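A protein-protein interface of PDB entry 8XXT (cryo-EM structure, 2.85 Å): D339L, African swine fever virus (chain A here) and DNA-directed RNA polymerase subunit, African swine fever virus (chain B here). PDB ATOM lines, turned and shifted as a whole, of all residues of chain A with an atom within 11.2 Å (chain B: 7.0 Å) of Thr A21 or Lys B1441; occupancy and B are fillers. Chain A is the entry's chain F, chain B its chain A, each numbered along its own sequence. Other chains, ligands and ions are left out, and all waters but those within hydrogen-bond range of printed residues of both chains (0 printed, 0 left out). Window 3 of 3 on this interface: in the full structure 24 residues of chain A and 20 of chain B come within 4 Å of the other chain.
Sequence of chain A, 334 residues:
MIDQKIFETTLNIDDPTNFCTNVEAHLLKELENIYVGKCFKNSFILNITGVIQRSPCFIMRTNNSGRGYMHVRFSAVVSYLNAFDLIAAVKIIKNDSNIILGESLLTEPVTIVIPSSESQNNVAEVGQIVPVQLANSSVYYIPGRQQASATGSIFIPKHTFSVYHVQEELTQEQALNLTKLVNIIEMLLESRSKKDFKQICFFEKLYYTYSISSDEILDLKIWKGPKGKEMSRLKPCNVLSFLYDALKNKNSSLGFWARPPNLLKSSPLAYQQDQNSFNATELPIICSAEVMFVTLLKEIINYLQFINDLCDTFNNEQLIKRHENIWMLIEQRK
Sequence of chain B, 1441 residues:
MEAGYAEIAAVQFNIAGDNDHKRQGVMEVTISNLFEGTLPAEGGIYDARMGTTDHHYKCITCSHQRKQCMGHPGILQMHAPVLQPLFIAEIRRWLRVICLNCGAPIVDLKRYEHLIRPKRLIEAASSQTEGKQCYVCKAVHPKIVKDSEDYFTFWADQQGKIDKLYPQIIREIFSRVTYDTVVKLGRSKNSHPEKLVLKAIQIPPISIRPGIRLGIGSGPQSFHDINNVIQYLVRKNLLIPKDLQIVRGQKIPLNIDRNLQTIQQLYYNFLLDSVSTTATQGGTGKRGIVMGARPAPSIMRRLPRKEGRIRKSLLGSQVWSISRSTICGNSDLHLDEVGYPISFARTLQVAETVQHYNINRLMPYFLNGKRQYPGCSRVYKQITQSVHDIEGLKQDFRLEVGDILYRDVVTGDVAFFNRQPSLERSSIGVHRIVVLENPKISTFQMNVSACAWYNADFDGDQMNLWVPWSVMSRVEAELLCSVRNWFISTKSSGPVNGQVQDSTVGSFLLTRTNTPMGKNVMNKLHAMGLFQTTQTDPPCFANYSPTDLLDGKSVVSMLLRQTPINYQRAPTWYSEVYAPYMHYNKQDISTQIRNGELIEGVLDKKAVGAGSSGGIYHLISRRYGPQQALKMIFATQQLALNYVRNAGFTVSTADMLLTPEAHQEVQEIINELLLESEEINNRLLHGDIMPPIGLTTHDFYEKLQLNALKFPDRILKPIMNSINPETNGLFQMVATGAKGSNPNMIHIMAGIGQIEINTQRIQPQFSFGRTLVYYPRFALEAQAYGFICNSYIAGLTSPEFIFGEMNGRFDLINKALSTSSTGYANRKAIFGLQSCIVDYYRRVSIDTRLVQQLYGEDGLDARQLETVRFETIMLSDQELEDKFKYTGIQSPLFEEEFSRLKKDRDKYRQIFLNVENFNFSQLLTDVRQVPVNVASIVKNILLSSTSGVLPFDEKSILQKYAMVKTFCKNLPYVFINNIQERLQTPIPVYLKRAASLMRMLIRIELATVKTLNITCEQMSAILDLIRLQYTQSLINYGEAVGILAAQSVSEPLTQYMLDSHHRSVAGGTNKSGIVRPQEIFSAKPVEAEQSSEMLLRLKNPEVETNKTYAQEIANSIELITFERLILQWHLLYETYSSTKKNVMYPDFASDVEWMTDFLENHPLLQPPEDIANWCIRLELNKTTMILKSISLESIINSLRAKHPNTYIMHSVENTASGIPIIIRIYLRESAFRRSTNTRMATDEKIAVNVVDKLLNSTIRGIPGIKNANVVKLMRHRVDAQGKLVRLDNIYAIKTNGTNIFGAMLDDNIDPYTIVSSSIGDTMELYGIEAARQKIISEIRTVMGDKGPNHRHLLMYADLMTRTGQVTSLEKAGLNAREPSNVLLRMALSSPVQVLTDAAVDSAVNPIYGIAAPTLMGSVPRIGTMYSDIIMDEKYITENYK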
ATOM      1  N   ILE A  13      -9.560 -17.050   2.800  1.00  0.00           N
ATOM      2  CA  ILE A  13      -8.422 -17.595   3.519  1.00  0.00           C
ATOM      3  C   ILE A  13      -7.327 -17.844   2.493  1.00  0.00           C
ATOM      4  O   ILE A  13      -7.378 -18.815   1.732  1.00  0.00           O
ATOM      5  CB  ILE A  13      -8.802 -18.866   4.278  1.00  0.00           C
ATOM      6  CG1 ILE A  13      -9.885 -18.541   5.301  1.00  0.00           C
ATOM      7  CG2 ILE A  13      -7.603 -19.437   4.964  1.00  0.00           C
ATOM      8  CD1 ILE A  13     -10.501 -19.740   5.926  1.00  0.00           C
ATOM      9  N   ASP A  15      -4.179 -18.615   3.029  1.00  0.00           N
ATOM     10  CA  ASP A  15      -3.303 -19.714   3.434  1.00  0.00           C
ATOM     11  C   ASP A  15      -4.089 -20.643   4.346  1.00  0.00           C
ATOM     12  O   ASP A  15      -3.971 -20.573   5.575  1.00  0.00           O
ATOM     13  CB  ASP A  15      -2.047 -19.190   4.130  1.00  0.00           C
ATOM     14  CG  ASP A  15      -0.975 -20.251   4.276  1.00  0.00           C
ATOM     15  OD1 ASP A  15      -1.254 -21.430   3.980  1.00  0.00           O
ATOM     16  OD2 ASP A  15       0.149 -19.906   4.690  1.00  0.00           O
ATOM     17  N   PRO A  16      -4.911 -21.526   3.775  1.00  0.00           N
ATOM     18  CA  PRO A  16      -5.713 -22.429   4.616  1.00  0.00           C
ATOM     19  C   PRO A  16      -4.883 -23.359   5.483  1.00  0.00           C
ATOM     20  O   PRO A  16      -5.332 -23.736   6.572  1.00  0.00           O
ATOM     21  CB  PRO A  16      -6.553 -23.201   3.592  1.00  0.00           C
ATOM     22  CG  PRO A  16      -5.817 -23.071   2.311  1.00  0.00           C
ATOM     23  CD  PRO A  16      -5.144 -21.743   2.341  1.00  0.00           C
ATOM     24  N   THR A  17      -3.690 -23.748   5.033  1.00  0.00           N
ATOM     25  CA  THR A  17      -2.840 -24.621   5.838  1.00  0.00           C
ATOM     26  C   THR A  17      -2.367 -23.915   7.103  1.00  0.00           C
ATOM     27  O   THR A  17      -2.394 -24.491   8.195  1.00  0.00           O
ATOM     28  CB  THR A  17      -1.649 -25.097   5.010  1.00  0.00           C
ATOM     29  OG1 THR A  17      -1.533 -24.292   3.830  1.00  0.00           O
ATOM     30  CG2 THR A  17      -1.834 -26.547   4.609  1.00  0.00           C
ATOM     31  N   ASN A  18      -1.922 -22.665   6.974  1.00  0.00           N
ATOM     32  CA  ASN A  18      -1.490 -21.897   8.136  1.00  0.00           C
ATOM     33  C   ASN A  18      -2.669 -21.384   8.947  1.00  0.00           C
ATOM     34  O   ASN A  18      -2.533 -21.153  10.154  1.00  0.00           O
ATOM     35  CB  ASN A  18      -0.612 -20.728   7.693  1.00  0.00           C
ATOM     36  CG  ASN A  18      -0.060 -19.939   8.860  1.00  0.00           C
ATOM     37  OD1 ASN A  18       0.159 -20.478   9.941  1.00  0.00           O
ATOM     38  ND2 ASN A  18       0.170 -18.650   8.644  1.00  0.00           N
ATOM     39  N   PHE A  19      -3.821 -21.192   8.306  1.00  0.00           N
ATOM     40  CA  PHE A  19      -4.994 -20.687   9.007  1.00  0.00           C
ATOM     41  C   PHE A  19      -5.541 -21.718   9.985  1.00  0.00           C
ATOM     42  O   PHE A  19      -5.907 -21.384  11.117  1.00  0.00           O
ATOM     43  CB  PHE A  19      -6.064 -20.292   7.995  1.00  0.00           C
ATOM     44  CG  PHE A  19      -7.214 -19.541   8.585  1.00  0.00           C
ATOM     45  CD1 PHE A  19      -8.281 -20.210   9.145  1.00  0.00           C
ATOM     46  CD2 PHE A  19      -7.238 -18.159   8.559  1.00  0.00           C
ATOM     47  CE1 PHE A  19      -9.336 -19.521   9.682  1.00  0.00           C
ATOM     48  CE2 PHE A  19      -8.299 -17.466   9.094  1.00  0.00           C
ATOM     49  CZ  PHE A  19      -9.350 -18.150   9.654  1.00  0.00           C
ATOM     50  N   CYS A  20      -5.611 -22.980   9.564  1.00  0.00           N
ATOM     51  CA  CYS A  20      -6.240 -24.005  10.385  1.00  0.00           C
ATOM     52  C   CYS A  20      -5.393 -24.418  11.579  1.00  0.00           C
ATOM     53  O   CYS A  20      -5.888 -25.165  12.430  1.00  0.00           O
ATOM     54  CB  CYS A  20      -6.571 -25.230   9.535  1.00  0.00           C
ATOM     55  SG  CYS A  20      -8.102 -25.068   8.595  1.00  0.00           S
ATOM     56  N   THR A  21      -4.141 -23.964  11.663  1.00  0.00           N
ATOM     57  CA  THR A  21      -3.321 -24.276  12.828  1.00  0.00           C
ATOM     58  C   THR A  21      -3.932 -23.715  14.103  1.00  0.00           C
ATOM     59  O   THR A  21      -3.743 -24.281  15.184  1.00  0.00           O
ATOM     60  CB  THR A  21      -1.907 -23.738  12.637  1.00  0.00           C
ATOM     61  OG1 THR A  21      -1.954 -22.317  12.469  1.00  0.00           O
ATOM     62  CG2 THR A  21      -1.260 -24.368  11.417  1.00  0.00           C
ATOM     63  N   ASN A  22      -4.657 -22.604  14.000  1.00  0.00           N
ATOM     64  CA  ASN A  22      -5.443 -22.073  15.116  1.00  0.00           C
ATOM     65  C   ASN A  22      -6.673 -21.406  14.498  1.00  0.00           C
ATOM     66  O   ASN A  22      -6.637 -20.231  14.131  1.00  0.00           O
ATOM     67  CB  ASN A  22      -4.634 -21.102  15.963  1.00  0.00           C
ATOM     68  CG  ASN A  22      -5.281 -20.819  17.300  1.00  0.00           C
ATOM     69  OD1 ASN A  22      -6.468 -21.067  17.494  1.00  0.00           O
ATOM     70  ND2 ASN A  22      -4.497 -20.297  18.233  1.00  0.00           N
ATOM     71  N   VAL A  23      -7.754 -22.176  14.389  1.00  0.00           N
ATOM     72  CA  VAL A  23      -8.913 -21.719  13.629  1.00  0.00           C
ATOM     73  C   VAL A  23      -9.605 -20.565  14.336  1.00  0.00           C
ATOM     74  O   VAL A  23      -9.902 -19.535  13.724  1.00  0.00           O
ATOM     75  CB  VAL A  23      -9.886 -22.883  13.381  1.00  0.00           C
ATOM     76  CG1 VAL A  23     -11.186 -22.360  12.815  1.00  0.00           C
ATOM     77  CG2 VAL A  23      -9.262 -23.885  12.444  1.00  0.00           C
ATOM     78  N   GLU A  24      -9.871 -20.714  15.633  1.00  0.00           N
ATOM     79  CA  GLU A  24     -10.684 -19.727  16.333  1.00  0.00           C
ATOM     80  C   GLU A  24      -9.945 -18.404  16.488  1.00  0.00           C
ATOM     81  O   GLU A  24     -10.515 -17.334  16.245  1.00  0.00           O
ATOM     82  CB  GLU A  24     -11.110 -20.274  17.692  1.00  0.00           C
ATOM     83  CG  GLU A  24     -12.058 -21.452  17.595  1.00  0.00           C
ATOM     84  CD  GLU A  24     -13.277 -21.140  16.748  1.00  0.00           C
ATOM     85  OE1 GLU A  24     -13.861 -20.049  16.923  1.00  0.00           O
ATOM     86  OE2 GLU A  24     -13.648 -21.982  15.906  1.00  0.00           O
ATOM     87  N   ALA A  25      -8.673 -18.458  16.883  1.00  0.00           N
ATOM     88  CA  ALA A  25      -7.904 -17.233  17.065  1.00  0.00           C
ATOM     89  C   ALA A  25      -7.737 -16.489  15.748  1.00  0.00           C
ATOM     90  O   ALA A  25      -7.963 -15.276  15.674  1.00  0.00           O
ATOM     91  CB  ALA A  25      -6.543 -17.556  17.678  1.00  0.00           C
ATOM     92  N   HIS A  26      -7.338 -17.204  14.693  1.00  0.00           N
ATOM     93  CA  HIS A  26      -7.157 -16.567  13.394  1.00  0.00           C
ATOM     94  C   HIS A  26      -8.473 -16.025  12.860  1.00  0.00           C
ATOM     95  O   HIS A  26      -8.511 -14.945  12.260  1.00  0.00           O
ATOM     96  CB  HIS A  26      -6.543 -17.553  12.404  1.00  0.00           C
ATOM     97  CG  HIS A  26      -5.135 -17.936  12.731  1.00  0.00           C
ATOM     98  ND1 HIS A  26      -4.510 -19.024  12.165  1.00  0.00           N
ATOM     99  CD2 HIS A  26      -4.232 -17.375  13.567  1.00  0.00           C
ATOM    100  CE1 HIS A  26      -3.279 -19.116  12.636  1.00  0.00           C
ATOM    101  NE2 HIS A  26      -3.086 -18.127  13.489  1.00  0.00           N
ATOM    102  N   LEU A  27      -9.562 -16.764  13.066  1.00  0.00           N
ATOM    103  CA  LEU A  27     -10.875 -16.296  12.641  1.00  0.00           C
ATOM    104  C   LEU A  27     -11.249 -15.002  13.345  1.00  0.00           C
ATOM    105  O   LEU A  27     -11.735 -14.058  12.711  1.00  0.00           O
ATOM    106  CB  LEU A  27     -11.916 -17.377  12.916  1.00  0.00           C
ATOM    107  CG  LEU A  27     -13.217 -17.311  12.130  1.00  0.00           C
ATOM    108  CD1 LEU A  27     -12.927 -17.458  10.658  1.00  0.00           C
ATOM    109  CD2 LEU A  27     -14.147 -18.407  12.598  1.00  0.00           C
ATOM    110  N   LYS A  29      -9.203 -12.793  14.718  1.00  0.00           N
ATOM    111  CA  LYS A  29      -8.340 -11.709  14.258  1.00  0.00           C
ATOM    112  C   LYS A  29      -8.754 -11.211  12.879  1.00  0.00           C
ATOM    113  O   LYS A  29      -8.764 -10.001  12.629  1.00  0.00           O
ATOM    114  CB  LYS A  29      -6.881 -12.154  14.255  1.00  0.00           C
ATOM    115  CG  LYS A  29      -6.401 -12.665  15.596  1.00  0.00           C
ATOM    116  CD  LYS A  29      -6.536 -11.599  16.671  1.00  0.00           C
ATOM    117  CE  LYS A  29      -6.127 -12.136  18.033  1.00  0.00           C
ATOM    118  NZ  LYS A  29      -6.227 -13.620  18.096  1.00  0.00           N
ATOM    119  N   ARG A  54     -19.522 -21.491  12.433  1.00  0.00           N
ATOM    120  CA  ARG A  54     -18.620 -21.342  11.306  1.00  0.00           C
ATOM    121  C   ARG A  54     -18.703 -22.594  10.453  1.00  0.00           C
ATOM    122  O   ARG A  54     -19.138 -23.652  10.908  1.00  0.00           O
ATOM    123  CB  ARG A  54     -17.181 -21.087  11.760  1.00  0.00           C
ATOM    124  CG  ARG A  54     -16.745 -21.936  12.932  1.00  0.00           C
ATOM    125  CD  ARG A  54     -15.239 -21.970  13.041  1.00  0.00           C
ATOM    126  NE  ARG A  54     -14.638 -22.615  11.884  1.00  0.00           N
ATOM    127  CZ  ARG A  54     -14.120 -23.835  11.895  1.00  0.00           C
ATOM    128  NH1 ARG A  54     -14.106 -24.569  12.995  1.00  0.00           N
ATOM    129  NH2 ARG A  54     -13.600 -24.329  10.776  1.00  0.00           N
ATOM    130  N   CYS A  57     -13.381 -25.097   6.672  1.00  0.00           N
ATOM    131  CA  CYS A  57     -12.611 -24.263   5.760  1.00  0.00           C
ATOM    132  C   CYS A  57     -12.608 -24.879   4.369  1.00  0.00           C
ATOM    133  O   CYS A  57     -11.730 -25.680   4.038  1.00  0.00           O
ATOM    134  CB  CYS A  57     -11.182 -24.078   6.266  1.00  0.00           C
ATOM    135  SG  CYS A  57     -10.130 -23.126   5.156  1.00  0.00           S
ATOM    136  N   MET A  70     -14.535 -20.360   3.861  1.00  0.00           N
ATOM    137  CA  MET A  70     -15.175 -20.552   5.162  1.00  0.00           C
ATOM    138  C   MET A  70     -16.199 -19.471   5.493  1.00  0.00           C
ATOM    139  O   MET A  70     -15.903 -18.274   5.433  1.00  0.00           O
ATOM    140  CB  MET A  70     -14.139 -20.639   6.285  1.00  0.00           C
ATOM    141  CG  MET A  70     -14.667 -20.173   7.629  1.00  0.00           C
ATOM    142  SD  MET A  70     -14.094 -21.168   9.008  1.00  0.00           S
ATOM    143  CE  MET A  70     -12.384 -20.695   9.057  1.00  0.00           C
ATOM    144  N   GLU B1433      -8.909 -29.519  10.035  1.00  0.00           N
ATOM    145  CA  GLU B1433      -8.479 -28.737  11.188  1.00  0.00           C
ATOM    146  C   GLU B1433      -7.836 -29.623  12.247  1.00  0.00           C
ATOM    147  O   GLU B1433      -6.807 -29.260  12.828  1.00  0.00           O
ATOM    148  CB  GLU B1433      -9.667 -27.981  11.778  1.00  0.00           C
ATOM    149  CG  GLU B1433     -10.241 -26.918  10.867  1.00  0.00           C
ATOM    150  CD  GLU B1433     -11.730 -26.737  11.054  1.00  0.00           C
ATOM    151  OE1 GLU B1433     -12.223 -26.969  12.176  1.00  0.00           O
ATOM    152  OE2 GLU B1433     -12.409 -26.348  10.084  1.00  0.00           O
ATOM    153  N   TYR B1435      -6.320 -32.537  11.882  1.00  0.00           N
ATOM    154  CA  TYR B1435      -5.034 -33.075  11.457  1.00  0.00           C
ATOM    155  C   TYR B1435      -3.964 -31.993  11.407  1.00  0.00           C
ATOM    156  O   TYR B1435      -2.818 -32.231  11.803  1.00  0.00           O
ATOM    157  CB  TYR B1435      -5.174 -33.750  10.097  1.00  0.00           C
ATOM    158  CG  TYR B1435      -3.941 -34.492   9.656  1.00  0.00           C
ATOM    159  CD1 TYR B1435      -3.579 -35.688  10.251  1.00  0.00           C
ATOM    160  CD2 TYR B1435      -3.139 -33.997   8.642  1.00  0.00           C
ATOM    161  CE1 TYR B1435      -2.453 -36.367   9.850  1.00  0.00           C
ATOM    162  CE2 TYR B1435      -2.013 -34.670   8.234  1.00  0.00           C
ATOM    163  CZ  TYR B1435      -1.674 -35.853   8.841  1.00  0.00           C
ATOM    164  OH  TYR B1435      -0.550 -36.529   8.438  1.00  0.00           O
ATOM    165  N   ILE B1436      -4.312 -30.802  10.917  1.00  0.00           N
ATOM    166  CA  ILE B1436      -3.327 -29.729  10.809  1.00  0.00           C
ATOM    167  C   ILE B1436      -2.887 -29.266  12.192  1.00  0.00           C
ATOM    168  O   ILE B1436      -1.715 -28.938  12.409  1.00  0.00           O
ATOM    169  CB  ILE B1436      -3.892 -28.568   9.974  1.00  0.00           C
ATOM    170  CG1 ILE B1436      -4.013 -28.979   8.510  1.00  0.00           C
ATOM    171  CG2 ILE B1436      -3.014 -27.340  10.091  1.00  0.00           C
ATOM    172  CD1 ILE B1436      -4.975 -28.132   7.732  1.00  0.00           C
ATOM    173  N   THR B1437      -3.816 -29.237  13.148  1.00  0.00           N
ATOM    174  CA  THR B1437      -3.471 -28.819  14.501  1.00  0.00           C
ATOM    175  C   THR B1437      -2.453 -29.763  15.130  1.00  0.00           C
ATOM    176  O   THR B1437      -1.510 -29.318  15.794  1.00  0.00           O
ATOM    177  CB  THR B1437      -4.729 -28.747  15.362  1.00  0.00           C
ATOM    178  OG1 THR B1437      -5.757 -28.057  14.643  1.00  0.00           O
ATOM    179  CG2 THR B1437      -4.443 -28.002  16.650  1.00  0.00           C
ATOM    180  N   GLU B1438      -2.626 -31.069  14.936  1.00  0.00           N
ATOM    181  CA  GLU B1438      -1.711 -32.022  15.554  1.00  0.00           C
ATOM    182  C   GLU B1438      -0.365 -32.057  14.844  1.00  0.00           C
ATOM    183  O   GLU B1438       0.683 -32.117  15.496  1.00  0.00           O
ATOM    184  CB  GLU B1438      -2.335 -33.415  15.567  1.00  0.00           C
ATOM    185  CG  GLU B1438      -3.727 -33.474  16.157  1.00  0.00           C
ATOM    186  CD  GLU B1438      -4.486 -34.709  15.714  1.00  0.00           C
ATOM    187  OE1 GLU B1438      -3.866 -35.587  15.078  1.00  0.00           O
ATOM    188  OE2 GLU B1438      -5.700 -34.800  15.994  1.00  0.00           O
ATOM    189  N   ASN B1439      -0.365 -32.015  13.513  1.00  0.00           N
ATOM    190  CA  ASN B1439       0.804 -32.396  12.733  1.00  0.00           C
ATOM    191  C   ASN B1439       1.453 -31.252  11.969  1.00  0.00           C
ATOM    192  O   ASN B1439       2.390 -31.499  11.204  1.00  0.00           O
ATOM    193  CB  ASN B1439       0.426 -33.506  11.751  1.00  0.00           C
ATOM    194  CG  ASN B1439      -0.191 -34.702  12.438  1.00  0.00           C
ATOM    195  OD1 ASN B1439       0.508 -35.615  12.871  1.00  0.00           O
ATOM    196  ND2 ASN B1439      -1.511 -34.699  12.550  1.00  0.00           N
ATOM    197  N   TYR B1440       0.993 -30.012  12.138  1.00  0.00           N
ATOM    198  CA  TYR B1440       1.558 -28.900  11.388  1.00  0.00           C
ATOM    199  C   TYR B1440       1.868 -27.673  12.233  1.00  0.00           C
ATOM    200  O   TYR B1440       2.381 -26.688  11.691  1.00  0.00           O
ATOM    201  CB  TYR B1440       0.618 -28.494  10.242  1.00  0.00           C
ATOM    202  CG  TYR B1440       0.737 -29.368   9.018  1.00  0.00           C
ATOM    203  CD1 TYR B1440       0.173 -30.634   8.990  1.00  0.00           C
ATOM    204  CD2 TYR B1440       1.414 -28.927   7.893  1.00  0.00           C
ATOM    205  CE1 TYR B1440       0.282 -31.437   7.877  1.00  0.00           C
ATOM    206  CE2 TYR B1440       1.528 -29.725   6.773  1.00  0.00           C
ATOM    207  CZ  TYR B1440       0.960 -30.978   6.771  1.00  0.00           C
ATOM    208  OH  TYR B1440       1.071 -31.777   5.658  1.00  0.00           O
ATOM    209  N   LYS B1441       1.580 -27.698  13.529  1.00  0.00           N
ATOM    210  CA  LYS B1441       1.837 -26.546  14.384  1.00  0.00           C
ATOM    211  C   LYS B1441       3.332 -26.277  14.527  1.00  0.00           C
ATOM    212  O   LYS B1441       3.788 -25.149  14.346  1.00  0.00           O
ATOM    213  CB  LYS B1441       1.206 -26.747  15.764  1.00  0.00           C
ATOM    214  CG  LYS B1441      -0.286 -26.464  15.823  1.00  0.00           C
ATOM    215  CD  LYS B1441      -0.606 -24.976  15.738  1.00  0.00           C
ATOM    216  CE  LYS B1441       0.436 -24.103  16.430  1.00  0.00           C
ATOM    217  NZ  LYS B1441       0.447 -22.724  15.872  1.00  0.00           N
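OE2 of Glu B1433 is in salt-bridge range of NH2 of Arg A54 (2.4 Å).
The backbone carbonyl oxygen (O) of Glu B1433 is in hydrogen-bond range of the side-chain hydroxyl (OG1) of Thr B1437 (2.4 Å). The side-chain hydroxyl (OG1) of Thr A17 is in hydrogen-bond range of the side-chain carboxylate (OD1) of Asp A15, 2.9 Å away. The backbone carbonyl oxygen of Pro A16 lies close to the side-chain sulfur of Cys A20, 3.7 Å away. OG1 of Thr A21 is in hydrogen-bond range of O of Asn A18 (2.7 Å). OE2 of Glu A24 lies within salt-bridge range of NH1 of Arg A54 (3.9 Å). The guanidinium group (NE) of Arg A54 lies within hydrogen-bond range of the side-chain sulfur (SD) of Met A70.
Thr A17 touches Ile B1436 (O to CG2, 3.5 Å). Cys A20 touches Glu B1433 (SG to CG, 3.6 Å). CD1 of Ile B1436 touches CB of Cys A20 (3.8 Å). Thr B1437 touches Cys A20 (OG1 to O, 3.6 Å). CG2 of Ile B1436 touches CG2 of Thr A21, 3.7 Å away. CD of Lys B1441 touches O of Thr A21, 3.3 Å away. CG2 of Val A23 touches CG of Glu B1433 (3.6 Å). N of Cys A57 touches OE2 of Glu B1433, 3.8 Å away.
Printed residues of chain B within 4 Å of Thr A17: Ile B1436. Printed residues of chain B within 4 Å of Cys A20: Glu B1433, Ile B1436 and Thr B1437. Of chain B, only Ile B1436 and Lys B1441 come within 4 Å of Thr A21. Printed residues of chain B within 4 Å of Val A23: Glu B1433 (3.6 Å). Of the printed residues of chain B, Arg A54 touches Glu B1433. Tyr B1435 touches none of the printed residues of chain A. Thr B1437 touches one residue of chain A. Lys B1441 touches just one residue of chain A: Thr A21 (3.3 Å). The nearest residue of chain B that does not touch Thr A21 is Thr B1437 (4.1 Å). The nearest printed residue of chain B that does not touch Thr A17 is Tyr B1440 (5.1 Å).
Of the 18 printed residues of chain A, 6 touch a printed residue of chain B. Printed residues of chain A that touch a printed residue of chain B: Thr A17, Cys A20, Thr A21, Val A23, Arg A54 and Cys A57. Hydrophobic or aromatic side chains of chain A that line the printed part of chain B: Val A23. Of the 8 printed residues of chain B, 4 touch a printed residue of chain A. Printed residues of chain B that touch a printed residue of chain A: Glu B1433, Ile B1436, Thr B1437 and Lys B1441. Hydrophobic or aromatic side chains of chain B that line the printed part of chain A: Ile B1436. Among the printed residues, 9 pairs touch across the chains. Among the printed residues, Asp or Glu carboxylates within 4 Å of a Lys or Arg side-chain nitrogen of the other chain: Arg A54 with Glu B1433.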
